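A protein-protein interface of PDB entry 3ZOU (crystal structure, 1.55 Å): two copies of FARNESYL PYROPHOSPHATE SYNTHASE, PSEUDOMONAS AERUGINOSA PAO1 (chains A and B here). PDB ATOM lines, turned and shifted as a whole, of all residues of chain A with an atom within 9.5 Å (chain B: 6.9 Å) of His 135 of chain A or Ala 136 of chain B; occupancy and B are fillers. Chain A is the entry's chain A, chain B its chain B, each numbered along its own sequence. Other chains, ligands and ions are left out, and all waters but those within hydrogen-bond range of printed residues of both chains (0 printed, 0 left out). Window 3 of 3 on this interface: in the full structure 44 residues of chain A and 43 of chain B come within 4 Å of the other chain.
The backbone carbonyl oxygen of Glu 134 of chain B sits at hydrogen-bond distance from the side-chain sulfur of Cys 138 of chain B.
The backbone carbonyl oxygen (O) of Asn 131 of chain A sits at hydrogen-bond distance from the side-chain sulfur (SG) of Cys 138 of chain A (3.3 Å).
The backbone carbonyl oxygen (O) of Gln 133 of chain A is in hydrogen-bond range of the side-chain sulfur (SG) of Cys 138 of chain A.
The backbone carbonyl oxygen (O) of Leu 139 of chain A is in hydrogen-bond range of the side-chain hydroxyl (OG1) of Thr 143 of chain A (3.1 Å).
SG of Cys 138 of chain B is in hydrogen-bond range of O of Gln 133 of chain B.
O of Glu 134 of chain A lies within hydrogen-bond range of SG of Cys 138 of chain A (3.6 Å).
Of the 18 printed residues of chain A, 6 touch a printed residue of chain B.
Printed residues of chain A that touch a printed residue of chain B: Ala 126, His 135, Ala 136, Cys 138, Leu 139 and Leu 142.
Hydrophobic or aromatic side chains of chain A that line the printed part of chain B: Ala 126, His 135, Ala 136, Leu 139 and Leu 142.
Of the 9 printed residues of chain B, 4 touch a printed residue of chain A.
Printed residues of chain B that touch a printed residue of chain A: His 135, Ala 136, Cys 138 and Leu 139.
Asn 131 of chain A touches none of the printed residues of chain B.
Printed residues of chain B within 4 Å of His 135 of chain A: His 135, Ala 136 and Leu 139.
Of the printed residues of chain B, Ala 136 of chain A touches His 135 (3.8 Å).
Printed residues of chain B within 4 Å of Leu 139 of chain A: His 135 (3.6 Å), Cys 138 (3.8 Å) and Leu 139 (3.7 Å).
Thr 143 of chain A touches none of the printed residues of chain B.
Of chain A, only His 135 comes within 4 Å of Ala 136 of chain B.
Printed residues of chain A within 4 Å of Cys 138 of chain B: Leu 139 (3.8 Å).
His 135 of chain B touches its own counterpart, His 135 of chain A.
His 135 of chain A touches Ala 136 of chain B, and with the chains exchanged Ala 136 of chain A touches His 135 of chain B.
Cys 138 of chain A touches Leu 139 of chain B, and with the chains exchanged Leu 139 of chain A touches Cys 138 of chain B.
Leu 139 of chain A touches its own counterpart, Leu 139 of chain B.
Of the 10 pairs that touch across the chains among the printed residues, 8 have their exchanged pair printed and touching as well.
Among the printed residues, pairs that only touch across the chains: Ala 126 of chain A with Leu 139 of chain B, His 135 of chain A with His 135 of chain B, His 135 of chain A with Ala 136 of chain B, His 135 of chain A with Leu 139 of chain B, Ala 136 of chain A with His 135 of chain B, Cys 138 of chain A with Leu 139 of chain B, Leu 139 of chain A with His 135 of chain B, Leu 139 of chain A with Cys 138 of chain B, Leu 139 of chain A with Leu 139 of chain B and Leu 142 of chain A with Leu 139 of chain B.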
ATOM      1  N   LEU A 125      -6.431  26.922  11.329  1.00  0.00           N
ATOM      2  CA  LEU A 125      -6.450  25.464  11.506  1.00  0.00           C
ATOM      3  C   LEU A 125      -7.543  24.800  10.746  1.00  0.00           C
ATOM      4  O   LEU A 125      -7.429  23.617  10.417  1.00  0.00           O
ATOM      5  CB  LEU A 125      -6.552  25.074  13.001  1.00  0.00           C
ATOM      6  CG  LEU A 125      -5.392  25.419  13.852  1.00  0.00           C
ATOM      7  CD1 LEU A 125      -5.672  24.967  15.299  1.00  0.00           C
ATOM      8  CD2 LEU A 125      -4.150  24.712  13.322  1.00  0.00           C
ATOM      9  N   ALA A 126      -8.706  25.467  10.632  1.00  0.00           N
ATOM     10  CA  ALA A 126      -9.836  24.865   9.913  1.00  0.00           C
ATOM     11  C   ALA A 126      -9.724  24.936   8.417  1.00  0.00           C
ATOM     12  O   ALA A 126     -10.518  24.317   7.734  1.00  0.00           O
ATOM     13  CB  ALA A 126     -11.089  25.590  10.300  1.00  0.00           C
ATOM     14  N   ASP A 127      -8.834  25.789   7.926  1.00  0.00           N
ATOM     15  CA  ASP A 127      -8.530  26.016   6.469  1.00  0.00           C
ATOM     16  C   ASP A 127      -7.707  24.893   5.944  1.00  0.00           C
ATOM     17  O   ASP A 127      -6.568  24.771   6.272  1.00  0.00           O
ATOM     18  CB  ASP A 127      -7.739  27.354   6.351  1.00  0.00           C
ATOM     19  CG  ASP A 127      -7.479  27.801   4.929  1.00  0.00           C
ATOM     20  OD1 ASP A 127      -7.216  26.945   4.039  1.00  0.00           O
ATOM     21  OD2 ASP A 127      -7.563  29.032   4.700  1.00  0.00           O
ATOM     22  N   THR A 128      -8.325  24.029   5.148  1.00  0.00           N
ATOM     23  CA  THR A 128      -7.588  22.826   4.706  1.00  0.00           C
ATOM     24  C   THR A 128      -6.598  23.099   3.587  1.00  0.00           C
ATOM     25  O   THR A 128      -5.814  22.201   3.249  1.00  0.00           O
ATOM     26  CB  THR A 128      -8.538  21.694   4.313  1.00  0.00           C
ATOM     27  OG1 THR A 128      -9.393  22.131   3.259  1.00  0.00           O
ATOM     28  CG2 THR A 128      -9.397  21.288   5.475  1.00  0.00           C
ATOM     29  N   ARG A 129      -6.559  24.306   3.046  1.00  0.00           N
ATOM     30  CA  ARG A 129      -5.438  24.675   2.163  1.00  0.00           C
ATOM     31  C   ARG A 129      -4.223  25.053   3.014  1.00  0.00           C
ATOM     32  O   ARG A 129      -3.119  24.580   2.795  1.00  0.00           O
ATOM     33  CB  ARG A 129      -5.842  25.808   1.189  1.00  0.00           C
ATOM     34  CG  ARG A 129      -4.721  26.230   0.233  1.00  0.00           C
ATOM     35  CD  ARG A 129      -5.058  27.468  -0.609  1.00  0.00           C
ATOM     36  NE  ARG A 129      -5.134  28.683   0.226  1.00  0.00           N
ATOM     37  CZ  ARG A 129      -4.084  29.341   0.727  1.00  0.00           C
ATOM     38  NH1 ARG A 129      -2.838  28.941   0.483  1.00  0.00           N
ATOM     39  NH2 ARG A 129      -4.286  30.406   1.496  1.00  0.00           N
ATOM     40  N   ASN A 131      -3.831  24.330   6.243  1.00  0.00           N
ATOM     41  CA  ASN A 131      -3.596  23.245   7.186  1.00  0.00           C
ATOM     42  C   ASN A 131      -4.019  21.909   6.566  1.00  0.00           C
ATOM     43  O   ASN A 131      -5.030  21.329   6.942  1.00  0.00           O
ATOM     44  CB  ASN A 131      -4.421  23.495   8.487  1.00  0.00           C
ATOM     45  CG  ASN A 131      -3.988  22.563   9.624  1.00  0.00           C
ATOM     46  OD1 ASN A 131      -2.823  22.100   9.672  1.00  0.00           O
ATOM     47  ND2 ASN A 131      -4.928  22.268  10.554  1.00  0.00           N
ATOM     48  N   PRO A 132      -3.195  21.427   5.606  1.00  0.00           N
ATOM     49  CA  PRO A 132      -3.665  20.319   4.765  1.00  0.00           C
ATOM     50  C   PRO A 132      -3.446  18.957   5.367  1.00  0.00           C
ATOM     51  O   PRO A 132      -2.757  18.085   4.763  1.00  0.00           O
ATOM     52  CB  PRO A 132      -2.840  20.493   3.490  1.00  0.00           C
ATOM     53  CG  PRO A 132      -1.595  21.087   3.934  1.00  0.00           C
ATOM     54  CD  PRO A 132      -1.942  21.982   5.136  1.00  0.00           C
ATOM     55  N   GLN A 133      -4.016  18.723   6.546  1.00  0.00           N
ATOM     56  CA  GLN A 133      -3.978  17.436   7.198  1.00  0.00           C
ATOM     57  C   GLN A 133      -5.171  16.666   6.805  1.00  0.00           C
ATOM     58  O   GLN A 133      -6.084  17.247   6.203  1.00  0.00           O
ATOM     59  CB  GLN A 133      -3.933  17.538   8.743  1.00  0.00           C
ATOM     60  CG  GLN A 133      -3.088  18.680   9.265  1.00  0.00           C
ATOM     61  CD  GLN A 133      -1.698  18.779   8.754  1.00  0.00           C
ATOM     62  OE1 GLN A 133      -1.028  17.755   8.552  1.00  0.00           O
ATOM     63  NE2 GLN A 133      -1.202  20.018   8.588  1.00  0.00           N
ATOM     64  N   GLU A 134      -5.210  15.379   7.190  1.00  0.00           N
ATOM     65  CA  GLU A 134      -6.446  14.646   7.103  1.00  0.00           C
ATOM     66  C   GLU A 134      -7.497  15.377   7.980  1.00  0.00           C
ATOM     67  O   GLU A 134      -7.183  15.946   8.996  1.00  0.00           O
ATOM     68  CB  GLU A 134      -6.268  13.263   7.633  1.00  0.00           C
ATOM     69  CG  GLU A 134      -5.400  12.429   6.691  1.00  0.00           C
ATOM     70  CD  GLU A 134      -6.220  11.766   5.593  1.00  0.00           C
ATOM     71  OE1 GLU A 134      -7.462  11.931   5.577  1.00  0.00           O
ATOM     72  OE2 GLU A 134      -5.611  11.076   4.739  1.00  0.00           O
ATOM     73  N   HIS A 135      -8.740  15.327   7.546  1.00  0.00           N
ATOM     74  CA  HIS A 135      -9.795  16.114   8.200  1.00  0.00           C
ATOM     75  C   HIS A 135      -9.936  15.806   9.638  1.00  0.00           C
ATOM     76  O   HIS A 135     -10.176  16.711  10.437  1.00  0.00           O
ATOM     77  CB  HIS A 135     -11.129  15.998   7.463  1.00  0.00           C
ATOM     78  CG  HIS A 135     -11.112  16.646   6.123  1.00  0.00           C
ATOM     79  ND1 HIS A 135     -12.082  16.426   5.161  1.00  0.00           N
ATOM     80  CD2 HIS A 135     -10.203  17.465   5.550  1.00  0.00           C
ATOM     81  CE1 HIS A 135     -11.759  17.096   4.071  1.00  0.00           C
ATOM     82  NE2 HIS A 135     -10.625  17.722   4.278  1.00  0.00           N
ATOM     83  N   ALA A 136      -9.888  14.538  10.039  1.00  0.00           N
ATOM     84  CA  ALA A 136     -10.021  14.226  11.412  1.00  0.00           C
ATOM     85  C   ALA A 136      -8.879  14.815  12.256  1.00  0.00           C
ATOM     86  O   ALA A 136      -9.054  15.118  13.425  1.00  0.00           O
ATOM     87  CB  ALA A 136     -10.042  12.711  11.570  1.00  0.00           C
ATOM     88  N   VAL A 137      -7.696  14.881  11.656  1.00  0.00           N
ATOM     89  CA  VAL A 137      -6.533  15.504  12.284  1.00  0.00           C
ATOM     90  C   VAL A 137      -6.751  17.015  12.446  1.00  0.00           C
ATOM     91  O   VAL A 137      -6.483  17.553  13.529  1.00  0.00           O
ATOM     92  CB  VAL A 137      -5.202  15.199  11.575  1.00  0.00           C
ATOM     93  CG1 VAL A 137      -4.072  15.975  12.185  1.00  0.00           C
ATOM     94  CG2 VAL A 137      -4.933  13.704  11.623  1.00  0.00           C
ATOM     95  N   CYS A 138      -7.246  17.680  11.411  1.00  0.00           N
ATOM     96  CA  CYS A 138      -7.546  19.125  11.563  1.00  0.00           C
ATOM     97  C   CYS A 138      -8.524  19.323  12.728  1.00  0.00           C
ATOM     98  O   CYS A 138      -8.334  20.236  13.529  1.00  0.00           O
ATOM     99  CB  CYS A 138      -8.161  19.678  10.311  1.00  0.00           C
ATOM    100  SG  CYS A 138      -7.140  19.572   8.811  1.00  0.00           S
ATOM    101  N   LEU A 139      -9.509  18.474  12.836  1.00  0.00           N
ATOM    102  CA  LEU A 139     -10.538  18.665  13.878  1.00  0.00           C
ATOM    103  C   LEU A 139      -9.936  18.454  15.280  1.00  0.00           C
ATOM    104  O   LEU A 139     -10.253  19.165  16.238  1.00  0.00           O
ATOM    105  CB  LEU A 139     -11.726  17.773  13.636  1.00  0.00           C
ATOM    106  CG  LEU A 139     -12.622  18.229  12.518  1.00  0.00           C
ATOM    107  CD1 LEU A 139     -13.626  17.152  12.129  1.00  0.00           C
ATOM    108  CD2 LEU A 139     -13.422  19.456  12.925  1.00  0.00           C
ATOM    109  N   GLU A 140      -9.049  17.467  15.388  1.00  0.00           N
ATOM    110  CA  GLU A 140      -8.357  17.210  16.651  1.00  0.00           C
ATOM    111  C   GLU A 140      -7.461  18.387  17.048  1.00  0.00           C
ATOM    112  O   GLU A 140      -7.413  18.784  18.233  1.00  0.00           O
ATOM    113  CB  GLU A 140      -7.582  15.850  16.605  1.00  0.00           C
ATOM    114  CG  GLU A 140      -6.926  15.536  17.911  1.00  0.00           C
ATOM    115  CD  GLU A 140      -7.855  15.235  19.082  1.00  0.00           C
ATOM    116  OE1 GLU A 140      -9.122  15.097  18.948  1.00  0.00           O
ATOM    117  OE2 GLU A 140      -7.347  15.156  20.236  1.00  0.00           O
ATOM    118  N   MET A 141      -6.795  18.963  16.080  1.00  0.00           N
ATOM    119  CA  MET A 141      -5.938  20.167  16.311  1.00  0.00           C
ATOM    120  C   MET A 141      -6.807  21.301  16.863  1.00  0.00           C
ATOM    121  O   MET A 141      -6.431  21.999  17.784  1.00  0.00           O
ATOM    122  CB  MET A 141      -5.212  20.599  15.006  1.00  0.00           C
ATOM    123  CG  MET A 141      -4.178  19.575  14.577  1.00  0.00           C
ATOM    124  SD  MET A 141      -3.509  19.944  12.959  1.00  0.00           S
ATOM    125  CE  MET A 141      -2.295  21.112  13.413  1.00  0.00           C
ATOM    126  N   LEU A 142      -7.939  21.494  16.232  1.00  0.00           N
ATOM    127  CA  LEU A 142      -8.881  22.578  16.642  1.00  0.00           C
ATOM    128  C   LEU A 142      -9.460  22.344  18.010  1.00  0.00           C
ATOM    129  O   LEU A 142      -9.490  23.259  18.805  1.00  0.00           O
ATOM    130  CB  LEU A 142     -10.014  22.642  15.658  1.00  0.00           C
ATOM    131  CG  LEU A 142      -9.655  23.308  14.402  1.00  0.00           C
ATOM    132  CD1 LEU A 142     -10.396  22.766  13.169  1.00  0.00           C
ATOM    133  CD2 LEU A 142      -9.941  24.795  14.534  1.00  0.00           C
ATOM    134  N   THR A 143      -9.889  21.102  18.279  1.00  0.00           N
ATOM    135  CA  THR A 143     -10.351  20.724  19.602  1.00  0.00           C
ATOM    136  C   THR A 143      -9.315  21.033  20.630  1.00  0.00           C
ATOM    137  O   THR A 143      -9.553  21.640  21.704  1.00  0.00           O
ATOM    138  CB  THR A 143     -10.670  19.220  19.633  1.00  0.00           C
ATOM    139  OG1 THR A 143     -11.866  19.024  18.923  1.00  0.00           O
ATOM    140  CG2 THR A 143     -10.865  18.712  21.052  1.00  0.00           C
ATOM    141  N   GLN B 133     -21.500  16.028  12.347  1.00  0.00           N
ATOM    142  CA  GLN B 133     -21.525  16.111  10.923  1.00  0.00           C
ATOM    143  C   GLN B 133     -20.385  15.376  10.317  1.00  0.00           C
ATOM    144  O   GLN B 133     -19.458  14.995  11.042  1.00  0.00           O
ATOM    145  CB  GLN B 133     -21.456  17.600  10.401  1.00  0.00           C
ATOM    146  CG  GLN B 133     -22.178  18.606  11.273  1.00  0.00           C
ATOM    147  CD  GLN B 133     -23.589  18.271  11.663  1.00  0.00           C
ATOM    148  OE1 GLN B 133     -24.329  17.683  10.877  1.00  0.00           O
ATOM    149  NE2 GLN B 133     -23.992  18.658  12.883  1.00  0.00           N
ATOM    150  N   GLU B 134     -20.389  15.220   8.995  1.00  0.00           N
ATOM    151  CA  GLU B 134     -19.235  14.718   8.299  1.00  0.00           C
ATOM    152  C   GLU B 134     -18.086  15.676   8.566  1.00  0.00           C
ATOM    153  O   GLU B 134     -18.275  16.877   8.706  1.00  0.00           O
ATOM    154  CB  GLU B 134     -19.453  14.643   6.802  1.00  0.00           C
ATOM    155  CG  GLU B 134     -20.500  13.591   6.411  1.00  0.00           C
ATOM    156  CD  GLU B 134     -19.916  12.259   6.038  1.00  0.00           C
ATOM    157  OE1 GLU B 134     -19.149  11.668   6.837  1.00  0.00           O
ATOM    158  OE2 GLU B 134     -20.226  11.821   4.899  1.00  0.00           O
ATOM    159  N   HIS B 135     -16.903  15.135   8.711  1.00  0.00           N
ATOM    160  CA  HIS B 135     -15.769  15.968   9.139  1.00  0.00           C
ATOM    161  C   HIS B 135     -15.511  17.126   8.215  1.00  0.00           C
ATOM    162  O   HIS B 135     -15.168  18.198   8.720  1.00  0.00           O
ATOM    163  CB  HIS B 135     -14.517  15.092   9.297  1.00  0.00           C
ATOM    164  CG  HIS B 135     -14.651  14.143  10.456  1.00  0.00           C
ATOM    165  ND1 HIS B 135     -13.734  13.146  10.698  1.00  0.00           N
ATOM    166  CD2 HIS B 135     -15.559  14.060  11.448  1.00  0.00           C
ATOM    167  CE1 HIS B 135     -14.076  12.488  11.785  1.00  0.00           C
ATOM    168  NE2 HIS B 135     -15.142  13.056  12.302  1.00  0.00           N
ATOM    169  N   ALA B 136     -15.659  16.988   6.899  1.00  0.00           N
ATOM    170  CA  ALA B 136     -15.460  18.097   5.982  1.00  0.00           C
ATOM    171  C   ALA B 136     -16.469  19.237   6.258  1.00  0.00           C
ATOM    172  O   ALA B 136     -16.110  20.414   6.147  1.00  0.00           O
ATOM    173  CB  ALA B 136     -15.582  17.706   4.560  1.00  0.00           C
ATOM    174  N   VAL B 137     -17.667  18.828   6.653  1.00  0.00           N
ATOM    175  CA  VAL B 137     -18.743  19.773   6.993  1.00  0.00           C
ATOM    176  C   VAL B 137     -18.378  20.497   8.272  1.00  0.00           C
ATOM    177  O   VAL B 137     -18.550  21.709   8.377  1.00  0.00           O
ATOM    178  CB  VAL B 137     -20.101  19.099   7.054  1.00  0.00           C
ATOM    179  CG1 VAL B 137     -21.168  20.062   7.560  1.00  0.00           C
ATOM    180  CG2 VAL B 137     -20.494  18.553   5.697  1.00  0.00           C
ATOM    181  N   CYS B 138     -17.882  19.780   9.274  1.00  0.00           N
ATOM    182  CA  CYS B 138     -17.504  20.377  10.574  1.00  0.00           C
ATOM    183  C   CYS B 138     -16.457  21.451  10.267  1.00  0.00           C
ATOM    184  O   CYS B 138     -16.549  22.554  10.778  1.00  0.00           O
ATOM    185  CB  CYS B 138     -16.959  19.361  11.527  1.00  0.00           C
ATOM    186  SG  CYS B 138     -18.085  18.126  12.132  1.00  0.00           S
ATOM    187  N   LEU B 139     -15.501  21.141   9.417  1.00  0.00           N
ATOM    188  CA  LEU B 139     -14.424  22.088   9.117  1.00  0.00           C
ATOM    189  C   LEU B 139     -14.944  23.311   8.369  1.00  0.00           C
ATOM    190  O   LEU B 139     -14.496  24.418   8.624  1.00  0.00           O
ATOM    191  CB  LEU B 139     -13.315  21.376   8.364  1.00  0.00           C
ATOM    192  CG  LEU B 139     -12.508  20.408   9.172  1.00  0.00           C
ATOM    193  CD1 LEU B 139     -11.601  19.542   8.322  1.00  0.00           C
ATOM    194  CD2 LEU B 139     -11.602  21.138  10.147  1.00  0.00           C
ATOM    195  N   GLU B 140     -15.898  23.119   7.458  1.00  0.00           N
ATOM    196  CA  GLU B 140     -16.513  24.243   6.751  1.00  0.00           C
ATOM    197  C   GLU B 140     -17.313  25.118   7.704  1.00  0.00           C
ATOM    198  O   GLU B 140     -17.274  26.365   7.608  1.00  0.00           O
ATOM    199  CB  GLU B 140     -17.360  23.736   5.593  1.00  0.00           C
ATOM    200  CG  GLU B 140     -18.006  24.845   4.780  1.00  0.00           C
ATOM    201  CD  GLU B 140     -17.041  25.752   4.007  1.00  0.00           C
ATOM    202  OE1 GLU B 140     -15.787  25.515   3.857  1.00  0.00           O
ATOM    203  OE2 GLU B 140     -17.531  26.787   3.477  1.00  0.00           O
ATOM    204  N   MET B 141     -17.991  24.504   8.643  1.00  0.00           N
ATOM    205  CA  MET B 141     -18.775  25.247   9.655  1.00  0.00           C
ATOM    206  C   MET B 141     -17.774  26.131  10.487  1.00  0.00           C
ATOM    207  O   MET B 141     -18.042  27.308  10.773  1.00  0.00           O
ATOM    208  CB  MET B 141     -19.505  24.333  10.604  1.00  0.00           C
ATOM    209  CG  MET B 141     -20.673  23.639   9.927  1.00  0.00           C
ATOM    210  SD  MET B 141     -21.394  22.387  10.952  1.00  0.00           S
ATOM    211  CE  MET B 141     -22.481  23.371  11.901  1.00  0.00           C
